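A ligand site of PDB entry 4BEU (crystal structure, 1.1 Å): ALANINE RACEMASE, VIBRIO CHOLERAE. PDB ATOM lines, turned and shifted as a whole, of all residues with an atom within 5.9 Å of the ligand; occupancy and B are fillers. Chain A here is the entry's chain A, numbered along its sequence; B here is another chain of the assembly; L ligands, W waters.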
ATOM      1  N   ILE A  49      24.523 -13.092  30.220  1.00  0.00           N
ATOM      2  CA  ILE A  49      24.500 -11.894  31.046  1.00  0.00           C
ATOM      3  C   ILE A  49      23.062 -11.530  31.399  1.00  0.00           C
ATOM      4  O   ILE A  49      22.217 -11.325  30.511  1.00  0.00           O
ATOM      5  CB  ILE A  49      25.237 -10.760  30.351  1.00  0.00           C
ATOM      6  CG1 ILE A  49      26.668 -11.180  29.982  1.00  0.00           C
ATOM      7  CG2 ILE A  49      25.239  -9.533  31.241  1.00  0.00           C
ATOM      8  CD1 ILE A  49      27.494 -11.695  31.174  1.00  0.00           C
ATOM      9  N   LYS A  51      22.087  -9.198  34.018  1.00  0.00           N
ATOM     10  CA  LYS A  51      21.987  -7.999  34.824  1.00  0.00           C
ATOM     11  C   LYS A  51      20.649  -7.291  34.595  1.00  0.00           C
ATOM     12  O   LYS A  51      19.951  -7.541  33.601  1.00  0.00           O
ATOM     13  CB  LYS A  51      23.170  -7.087  34.514  1.00  0.00           C
ATOM     14  CG  LYS A  51      23.124  -6.525  33.142  1.00  0.00           C
ATOM     15  CD  LYS A  51      24.463  -5.969  32.728  1.00  0.00           C
ATOM     16  CE  LYS A  51      24.402  -5.153  31.467  1.00  0.00           C
ATOM     17  NZ  LYS A  51      25.779  -5.093  30.847  1.00  0.00           N
ATOM     18  N   TYR A  55      17.648  -8.164  32.002  1.00  0.00           N
ATOM     19  CA  TYR A  55      17.277  -7.137  31.033  1.00  0.00           C
ATOM     20  C   TYR A  55      15.767  -6.865  31.098  1.00  0.00           C
ATOM     21  O   TYR A  55      15.113  -6.635  30.068  1.00  0.00           O
ATOM     22  CB  TYR A  55      17.734  -7.501  29.633  1.00  0.00           C
ATOM     23  CG  TYR A  55      19.221  -7.335  29.355  1.00  0.00           C
ATOM     24  CD1 TYR A  55      20.180  -7.859  30.224  1.00  0.00           C
ATOM     25  CD2 TYR A  55      19.681  -6.722  28.184  1.00  0.00           C
ATOM     26  CE1 TYR A  55      21.558  -7.742  29.925  1.00  0.00           C
ATOM     27  CE2 TYR A  55      21.024  -6.625  27.899  1.00  0.00           C
ATOM     28  CZ  TYR A  55      21.954  -7.114  28.767  1.00  0.00           C
ATOM     29  OH  TYR A  55      23.327  -7.038  28.526  1.00  0.00           O
ATOM     30  N   VAL A  97      29.460  -8.333  36.588  1.00  0.00           N
ATOM     31  CA  VAL A  97      29.894  -7.613  35.402  1.00  0.00           C
ATOM     32  C   VAL A  97      30.184  -6.138  35.620  1.00  0.00           C
ATOM     33  O   VAL A  97      30.388  -5.387  34.653  1.00  0.00           O
ATOM     34  CB  VAL A  97      28.924  -7.790  34.222  1.00  0.00           C
ATOM     35  CG1 VAL A  97      28.819  -9.268  33.847  1.00  0.00           C
ATOM     36  CG2 VAL A  97      27.574  -7.236  34.560  1.00  0.00           C
ATOM     37  N   LEU A 116      34.822  -8.574  39.630  1.00  0.00           N
ATOM     38  CA  LEU A 116      35.473  -7.978  38.478  1.00  0.00           C
ATOM     39  C   LEU A 116      36.240  -6.783  38.959  1.00  0.00           C
ATOM     40  O   LEU A 116      35.639  -5.777  39.375  1.00  0.00           O
ATOM     41  CB  LEU A 116      34.412  -7.481  37.482  1.00  0.00           C
ATOM     42  CG  LEU A 116      34.975  -6.884  36.191  1.00  0.00           C
ATOM     43  CD1 LEU A 116      35.718  -7.913  35.380  1.00  0.00           C
ATOM     44  CD2 LEU A 116      33.871  -6.252  35.365  1.00  0.00           C
ATOM     45  N   ARG A 150      36.064   2.362  32.389  1.00  0.00           N
ATOM     46  CA  ARG A 150      34.936   2.088  33.278  1.00  0.00           C
ATOM     47  C   ARG A 150      35.360   1.189  34.450  1.00  0.00           C
ATOM     48  O   ARG A 150      35.749   1.697  35.495  1.00  0.00           O
ATOM     49  CB  ARG A 150      33.752   1.526  32.476  1.00  0.00           C
ATOM     50  CG  ARG A 150      32.457   1.359  33.256  1.00  0.00           C
ATOM     51  CD  ARG A 150      31.293   0.938  32.341  1.00  0.00           C
ATOM     52  NE  ARG A 150      31.511  -0.410  31.836  1.00  0.00           N
ATOM     53  CZ  ARG A 150      30.573  -1.144  31.273  1.00  0.00           C
ATOM     54  NH1 ARG A 150      29.362  -0.664  31.063  1.00  0.00           N
ATOM     55  NH2 ARG A 150      30.834  -2.385  30.887  1.00  0.00           N
ATOM     56  N   ASN A 151      35.314  -0.134  34.294  1.00  0.00           N
ATOM     57  CA  ASN A 151      35.651  -1.032  35.400  1.00  0.00           C
ATOM     58  C   ASN A 151      37.109  -1.501  35.410  1.00  0.00           C
ATOM     59  O   ASN A 151      37.544  -2.161  36.350  1.00  0.00           O
ATOM     60  CB  ASN A 151      34.777  -2.288  35.338  1.00  0.00           C
ATOM     61  CG  ASN A 151      33.317  -1.974  35.489  1.00  0.00           C
ATOM     62  OD1 ASN A 151      32.887  -1.357  36.470  1.00  0.00           O
ATOM     63  ND2 ASN A 151      32.529  -2.392  34.517  1.00  0.00           N
ATOM     64  N   MET A 179      39.770  -9.827  31.114  1.00  0.00           N
ATOM     65  CA  MET A 179      38.723  -9.415  30.180  1.00  0.00           C
ATOM     66  C   MET A 179      38.909  -7.990  29.752  1.00  0.00           C
ATOM     67  O   MET A 179      39.627  -7.219  30.368  1.00  0.00           O
ATOM     68  CB  MET A 179      37.328  -9.616  30.825  1.00  0.00           C
ATOM     69  CG  MET A 179      37.059  -8.767  32.072  1.00  0.00           C
ATOM     70  SD  MET A 179      36.555  -7.045  31.692  1.00  0.00           S
ATOM     71  CE  MET A 179      34.836  -7.274  31.261  1.00  0.00           C
ATOM     72  N   HIS A 181      36.150  -5.019  27.299  1.00  0.00           N
ATOM     73  CA  HIS A 181      34.808  -4.772  26.787  1.00  0.00           C
ATOM     74  C   HIS A 181      34.907  -3.630  25.798  1.00  0.00           C
ATOM     75  O   HIS A 181      35.680  -2.691  26.003  1.00  0.00           O
ATOM     76  CB  HIS A 181      33.895  -4.403  27.952  1.00  0.00           C
ATOM     77  CG  HIS A 181      32.431  -4.345  27.622  1.00  0.00           C
ATOM     78  ND1 HIS A 181      31.672  -5.462  27.355  1.00  0.00           N
ATOM     79  CD2 HIS A 181      31.592  -3.296  27.598  1.00  0.00           C
ATOM     80  CE1 HIS A 181      30.411  -5.095  27.177  1.00  0.00           C
ATOM     81  NE2 HIS A 181      30.337  -3.785  27.317  1.00  0.00           N
ATOM     82  N   TYR A 185      30.016  -0.822  18.028  1.00  0.00           N
ATOM     83  CA  TYR A 185      29.815  -1.954  17.152  1.00  0.00           C
ATOM     84  C   TYR A 185      30.639  -1.798  15.873  1.00  0.00           C
ATOM     85  O   TYR A 185      30.206  -2.236  14.802  1.00  0.00           O
ATOM     86  CB  TYR A 185      28.347  -2.094  16.793  1.00  0.00           C
ATOM     87  CG  TYR A 185      27.363  -2.426  17.923  1.00  0.00           C
ATOM     88  CD1 TYR A 185      27.771  -2.886  19.176  1.00  0.00           C
ATOM     89  CD2 TYR A 185      26.005  -2.312  17.707  1.00  0.00           C
ATOM     90  CE1 TYR A 185      26.830  -3.197  20.179  1.00  0.00           C
ATOM     91  CE2 TYR A 185      25.072  -2.623  18.682  1.00  0.00           C
ATOM     92  CZ  TYR A 185      25.483  -3.069  19.922  1.00  0.00           C
ATOM     93  OH  TYR A 185      24.523  -3.373  20.882  1.00  0.00           O
ATOM     94  N   ALA A 220      34.008 -10.463  24.509  1.00  0.00           N
ATOM     95  CA  ALA A 220      32.906 -10.262  23.577  1.00  0.00           C
ATOM     96  C   ALA A 220      31.536 -10.146  24.219  1.00  0.00           C
ATOM     97  O   ALA A 220      31.082 -11.086  24.868  1.00  0.00           O
ATOM     98  CB  ALA A 220      32.879 -11.397  22.585  1.00  0.00           C
ATOM     99  N   ASN A 221      30.875  -9.036  23.985  1.00  0.00           N
ATOM    100  CA  ASN A 221      29.437  -8.884  24.164  1.00  0.00           C
ATOM    101  C   ASN A 221      28.702  -9.516  22.974  1.00  0.00           C
ATOM    102  O   ASN A 221      29.311 -10.191  22.141  1.00  0.00           O
ATOM    103  CB  ASN A 221      29.097  -7.409  24.345  1.00  0.00           C
ATOM    104  CG  ASN A 221      29.494  -6.548  23.150  1.00  0.00           C
ATOM    105  OD1 ASN A 221      29.974  -7.038  22.137  1.00  0.00           O
ATOM    106  ND2 ASN A 221      29.289  -5.244  23.279  1.00  0.00           N
ATOM    107  N   SER A 222      27.388  -9.332  22.914  1.00  0.00           N
ATOM    108  CA  SER A 222      26.608  -9.977  21.858  1.00  0.00           C
ATOM    109  C   SER A 222      27.104  -9.627  20.457  1.00  0.00           C
ATOM    110  O   SER A 222      27.337 -10.509  19.632  1.00  0.00           O
ATOM    111  CB  SER A 222      25.145  -9.564  21.949  1.00  0.00           C
ATOM    112  OG  SER A 222      24.530  -9.963  23.167  1.00  0.00           O
ATOM    113  N   TYR A 223      27.253  -8.342  20.210  1.00  0.00           N
ATOM    114  CA  TYR A 223      27.674  -7.850  18.906  1.00  0.00           C
ATOM    115  C   TYR A 223      28.996  -8.496  18.510  1.00  0.00           C
ATOM    116  O   TYR A 223      29.162  -9.032  17.396  1.00  0.00           O
ATOM    117  CB  TYR A 223      27.838  -6.310  18.894  1.00  0.00           C
ATOM    118  CG  TYR A 223      28.541  -5.926  17.611  1.00  0.00           C
ATOM    119  CD1 TYR A 223      27.843  -5.880  16.426  1.00  0.00           C
ATOM    120  CD2 TYR A 223      29.917  -5.730  17.567  1.00  0.00           C
ATOM    121  CE1 TYR A 223      28.483  -5.644  15.223  1.00  0.00           C
ATOM    122  CE2 TYR A 223      30.568  -5.487  16.360  1.00  0.00           C
ATOM    123  CZ  TYR A 223      29.840  -5.440  15.211  1.00  0.00           C
ATOM    124  OH  TYR A 223      30.489  -5.247  14.010  1.00  0.00           O
ATOM    125  N   ARG A 237      30.226 -13.171  26.436  1.00  0.00           N
ATOM    126  CA  ARG A 237      29.320 -12.570  27.420  1.00  0.00           C
ATOM    127  C   ARG A 237      28.102 -11.957  26.719  1.00  0.00           C
ATOM    128  O   ARG A 237      27.926 -10.746  26.732  1.00  0.00           O
ATOM    129  CB  ARG A 237      30.044 -11.501  28.226  1.00  0.00           C
ATOM    130  CG  ARG A 237      31.257 -11.964  29.035  1.00  0.00           C
ATOM    131  CD  ARG A 237      31.715 -10.856  29.998  1.00  0.00           C
ATOM    132  NE  ARG A 237      31.945  -9.581  29.312  1.00  0.00           N
ATOM    133  CZ  ARG A 237      33.061  -9.228  28.675  1.00  0.00           C
ATOM    134  NH1 ARG A 237      34.133 -10.005  28.647  1.00  0.00           N
ATOM    135  NH2 ARG A 237      33.110  -8.078  28.045  1.00  0.00           N
ATOM    136  N   PRO A 238      27.253 -12.777  26.091  1.00  0.00           N
ATOM    137  CA  PRO A 238      26.057 -12.228  25.461  1.00  0.00           C
ATOM    138  C   PRO A 238      25.003 -11.873  26.489  1.00  0.00           C
ATOM    139  O   PRO A 238      24.644 -12.715  27.337  1.00  0.00           O
ATOM    140  CB  PRO A 238      25.548 -13.392  24.616  1.00  0.00           C
ATOM    141  CG  PRO A 238      26.009 -14.604  25.347  1.00  0.00           C
ATOM    142  CD  PRO A 238      27.386 -14.222  25.872  1.00  0.00           C
ATOM    143  N   GLY A 239      24.474 -10.665  26.390  1.00  0.00           N
ATOM    144  CA  GLY A 239      23.250 -10.288  27.075  1.00  0.00           C
ATOM    145  C   GLY A 239      22.136 -10.039  26.073  1.00  0.00           C
ATOM    146  O   GLY A 239      21.326 -10.921  25.814  1.00  0.00           O
ATOM    147  N   GLY A 240      22.150  -8.839  25.500  1.00  0.00           N
ATOM    148  CA  GLY A 240      21.069  -8.369  24.659  1.00  0.00           C
ATOM    149  C   GLY A 240      20.598  -9.358  23.597  1.00  0.00           C
ATOM    150  O   GLY A 240      19.386  -9.514  23.405  1.00  0.00           O
ATOM    151  N   VAL A 241      21.482 -10.063  22.893  1.00  0.00           N
ATOM    152  CA  VAL A 241      21.035 -10.910  21.821  1.00  0.00           C
ATOM    153  C   VAL A 241      20.173 -12.066  22.316  1.00  0.00           C
ATOM    154  O   VAL A 241      19.244 -12.496  21.614  1.00  0.00           O
ATOM    155  CB  VAL A 241      22.223 -11.408  20.945  1.00  0.00           C
ATOM    156  CG1 VAL A 241      23.078 -12.419  21.680  1.00  0.00           C
ATOM    157  CG2 VAL A 241      21.709 -11.944  19.620  1.00  0.00           C
ATOM    158  N   ASP A 245      17.556  -8.240  21.689  1.00  0.00           N
ATOM    159  CA  ASP A 245      17.871  -6.830  21.527  1.00  0.00           C
ATOM    160  C   ASP A 245      19.334  -6.679  21.097  1.00  0.00           C
ATOM    161  O   ASP A 245      20.191  -6.233  21.882  1.00  0.00           O
ATOM    162  CB  ASP A 245      17.643  -6.024  22.814  1.00  0.00           C
ATOM    163  CG  ASP A 245      18.060  -4.566  22.656  1.00  0.00           C
ATOM    164  OD1 ASP A 245      18.029  -4.074  21.506  1.00  0.00           O
ATOM    165  OD2 ASP A 245      18.425  -3.895  23.642  1.00  0.00           O
ATOM    166  N   TYR B 276      30.234   3.858  26.462  1.00  0.00           N
ATOM    167  CA  TYR B 276      29.763   3.484  25.139  1.00  0.00           C
ATOM    168  C   TYR B 276      29.758   4.683  24.197  1.00  0.00           C
ATOM    169  O   TYR B 276      29.434   5.798  24.581  1.00  0.00           O
ATOM    170  CB  TYR B 276      28.369   2.920  25.240  1.00  0.00           C
ATOM    171  CG  TYR B 276      28.314   1.544  25.840  1.00  0.00           C
ATOM    172  CD1 TYR B 276      28.947   0.474  25.220  1.00  0.00           C
ATOM    173  CD2 TYR B 276      27.567   1.288  26.979  1.00  0.00           C
ATOM    174  CE1 TYR B 276      28.872  -0.804  25.742  1.00  0.00           C
ATOM    175  CE2 TYR B 276      27.463   0.011  27.494  1.00  0.00           C
ATOM    176  CZ  TYR B 276      28.117  -1.039  26.872  1.00  0.00           C
ATOM    177  OH  TYR B 276      28.002  -2.323  27.347  1.00  0.00           O
ATOM    178  N   MET B 324      24.044   0.672  31.696  1.00  0.00           N
ATOM    179  CA  MET B 324      22.884   0.073  32.331  1.00  0.00           C
ATOM    180  C   MET B 324      23.004   0.041  33.843  1.00  0.00           C
ATOM    181  O   MET B 324      22.008   0.246  34.558  1.00  0.00           O
ATOM    182  CB  MET B 324      22.673  -1.334  31.767  1.00  0.00           C
ATOM    183  CG  MET B 324      21.357  -2.004  32.202  1.00  0.00           C
ATOM    184  SD  MET B 324      21.051  -3.636  31.514  1.00  0.00           S
ATOM    185  CE  MET B 324      20.756  -3.257  29.816  1.00  0.00           C
ATOM    186  N   ASN B 325      24.223  -0.190  34.353  1.00  0.00           N
ATOM    187  CA  ASN B 325      24.436  -0.379  35.773  1.00  0.00           C
ATOM    188  C   ASN B 325      25.508   0.474  36.421  1.00  0.00           C
ATOM    189  O   ASN B 325      25.683   0.377  37.634  1.00  0.00           O
ATOM    190  CB  ASN B 325      24.799  -1.846  36.072  1.00  0.00           C
ATOM    191  CG  ASN B 325      23.694  -2.782  35.752  1.00  0.00           C
ATOM    192  OD1 ASN B 325      22.658  -2.810  36.451  1.00  0.00           O
ATOM    193  ND2 ASN B 325      23.857  -3.537  34.718  1.00  0.00           N
HETATM  194  N1  LIG L   1      29.905  -7.641  29.458  1.00  0.00           N
HETATM  195  C1  LIG L   1      29.824  -6.527  30.225  1.00  0.00           C
HETATM  196  C2  LIG L   1      31.036  -6.121  30.992  1.00  0.00           C
HETATM  197  C3  LIG L   1      28.631  -5.792  30.237  1.00  0.00           C
HETATM  198  O1  LIG L   1      28.567  -4.650  30.980  1.00  0.00           O
HETATM  199  C4  LIG L   1      27.525  -6.228  29.498  1.00  0.00           C
HETATM  200  C5  LIG L   1      26.132  -5.899  29.914  1.00  0.00           C
HETATM  201  C6  LIG L   1      27.632  -7.370  28.708  1.00  0.00           C
HETATM  202  C7  LIG L   1      28.835  -8.049  28.698  1.00  0.00           C
HETATM  203  C8  LIG L   1      26.484  -7.805  27.812  1.00  0.00           C
HETATM  204  O2  LIG L   1      26.362  -6.818  26.753  1.00  0.00           O
HETATM  205  P1  LIG L   1      25.319  -6.930  25.458  1.00  0.00           P
HETATM  206  O3  LIG L   1      23.924  -6.785  26.035  1.00  0.00           O
HETATM  207  O4  LIG L   1      25.552  -8.328  24.891  1.00  0.00           O
HETATM  208  O5  LIG L   1      25.735  -5.835  24.521  1.00  0.00           O
HETATM  209  O   HOH W   1      27.580  -3.980  25.133  1.00  0.00           O
HETATM  210  O   HOH W   2      24.288  -3.920  23.475  1.00  0.00           O
HETATM  211  O   HOH W   3      28.536  -3.786  33.441  1.00  0.00           O
HETATM  212  O   HOH W   4      26.302  -6.204  21.880  1.00  0.00           O
HETATM  213  O   HOH W   5      27.764  -2.396  29.855  1.00  0.00           O
HETATM  214  O   HOH W   6      23.680  -7.103  23.260  1.00  0.00           O
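NH2 of Arg 237 is in hydrogen-bond range of ND1 of His 181, at 3.1 Å.
The guanidinium group of Arg 150 sits close to the side-chain amide nitrogen of Asn 151.
N of Arg 237 sits at hydrogen-bond distance from O of Ala 220, 2.7 Å away.
The side-chain hydroxyl (OG) of Ser 222 is in hydrogen-bond range of the backbone NH (N) of Val 241, 3.1 Å away.
A ring nitrogen (NE2) of His 181 lies within hydrogen-bond range of the side-chain hydroxyl (OH) of Tyr 276 of chain B (2.8 Å).
OG of Ser 222 sits at hydrogen-bond distance from N of Gly 239, 3.3 Å away.
The backbone NH (N) of Ile 49 is in hydrogen-bond range of the backbone carbonyl oxygen (O) of Pro 238 (2.9 Å).
The backbone carbonyl oxygen of Gly 240 is in hydrogen-bond range of the backbone NH of Asp 245.
Ile 49 touches the ligand.
O of Val 97 touches C2 of the ligand, 3.8 Å away.
CE of Met 179 touches C2 of the ligand, 3.98 Å away.
CE1 of His 181 touches C1 of the ligand (3.4 Å).
CB of Asn 221 touches O2 of the ligand, at 3.7 Å.
Pro 238 touches the ligand (C to O4, 3.9 Å).
Hydrophobic or aromatic side chains that line the ligand: Ile 49, Tyr 55, Met 179 and His 181.
Along chain A the residues within 4 Å of the ligand span positions 49 to 240.
Water W3 lies within hydrogen-bond range of an oxygen (O1) of the ligand (2.6 Å) and the backbone carbonyl oxygen (O) of Val 97 (2.7 Å).
Water W2 bridges an oxygen (O5) of the ligand and the side-chain hydroxyl of Tyr 185.
Water W5 lies within hydrogen-bond range of OH of Tyr 276 of chain B (2.5 Å), O1 of the ligand (2.6 Å), NH1 of Arg 150 (2.6 Å) and NZ of Lys 51 (3.5 Å).
Water W1 lies within hydrogen-bond range of an oxygen (O5) of the ligand, the side-chain hydroxyl of Tyr 276 of chain B and the side-chain amide nitrogen of Asn 221.
Water W6 lies within hydrogen-bond range of an oxygen (O5) of the ligand (2.7 Å), the side-chain hydroxyl (OG) of Ser 222 (3.0 Å) and the backbone NH (N) of Gly 240 (3.2 Å).
OH of Tyr 55 sits at hydrogen-bond distance from O3 of the ligand (2.6 Å).
The backbone NH (N) of Gly 239 lies within hydrogen-bond range of an oxygen (O4) of the ligand (3.0 Å).
The side-chain hydroxyl (OG) of Ser 222 is in hydrogen-bond range of an oxygen (O4) of the ligand (2.6 Å).
The guanidinium group of Arg 150 is in hydrogen-bond range of an oxygen (O1) of the ligand.
An oxygen (O3) of the ligand is in hydrogen-bond range of the backbone NH (N) of Gly 240.
C5 of the ligand is covalently linked to NZ of Lys 51 (1.3 Å).
N1 of the ligand lies within hydrogen-bond range of NE of Arg 237 (2.8 Å).
An oxygen (O4) of the ligand is in hydrogen-bond range of the backbone NH (N) of Ser 222, 2.9 Å away.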
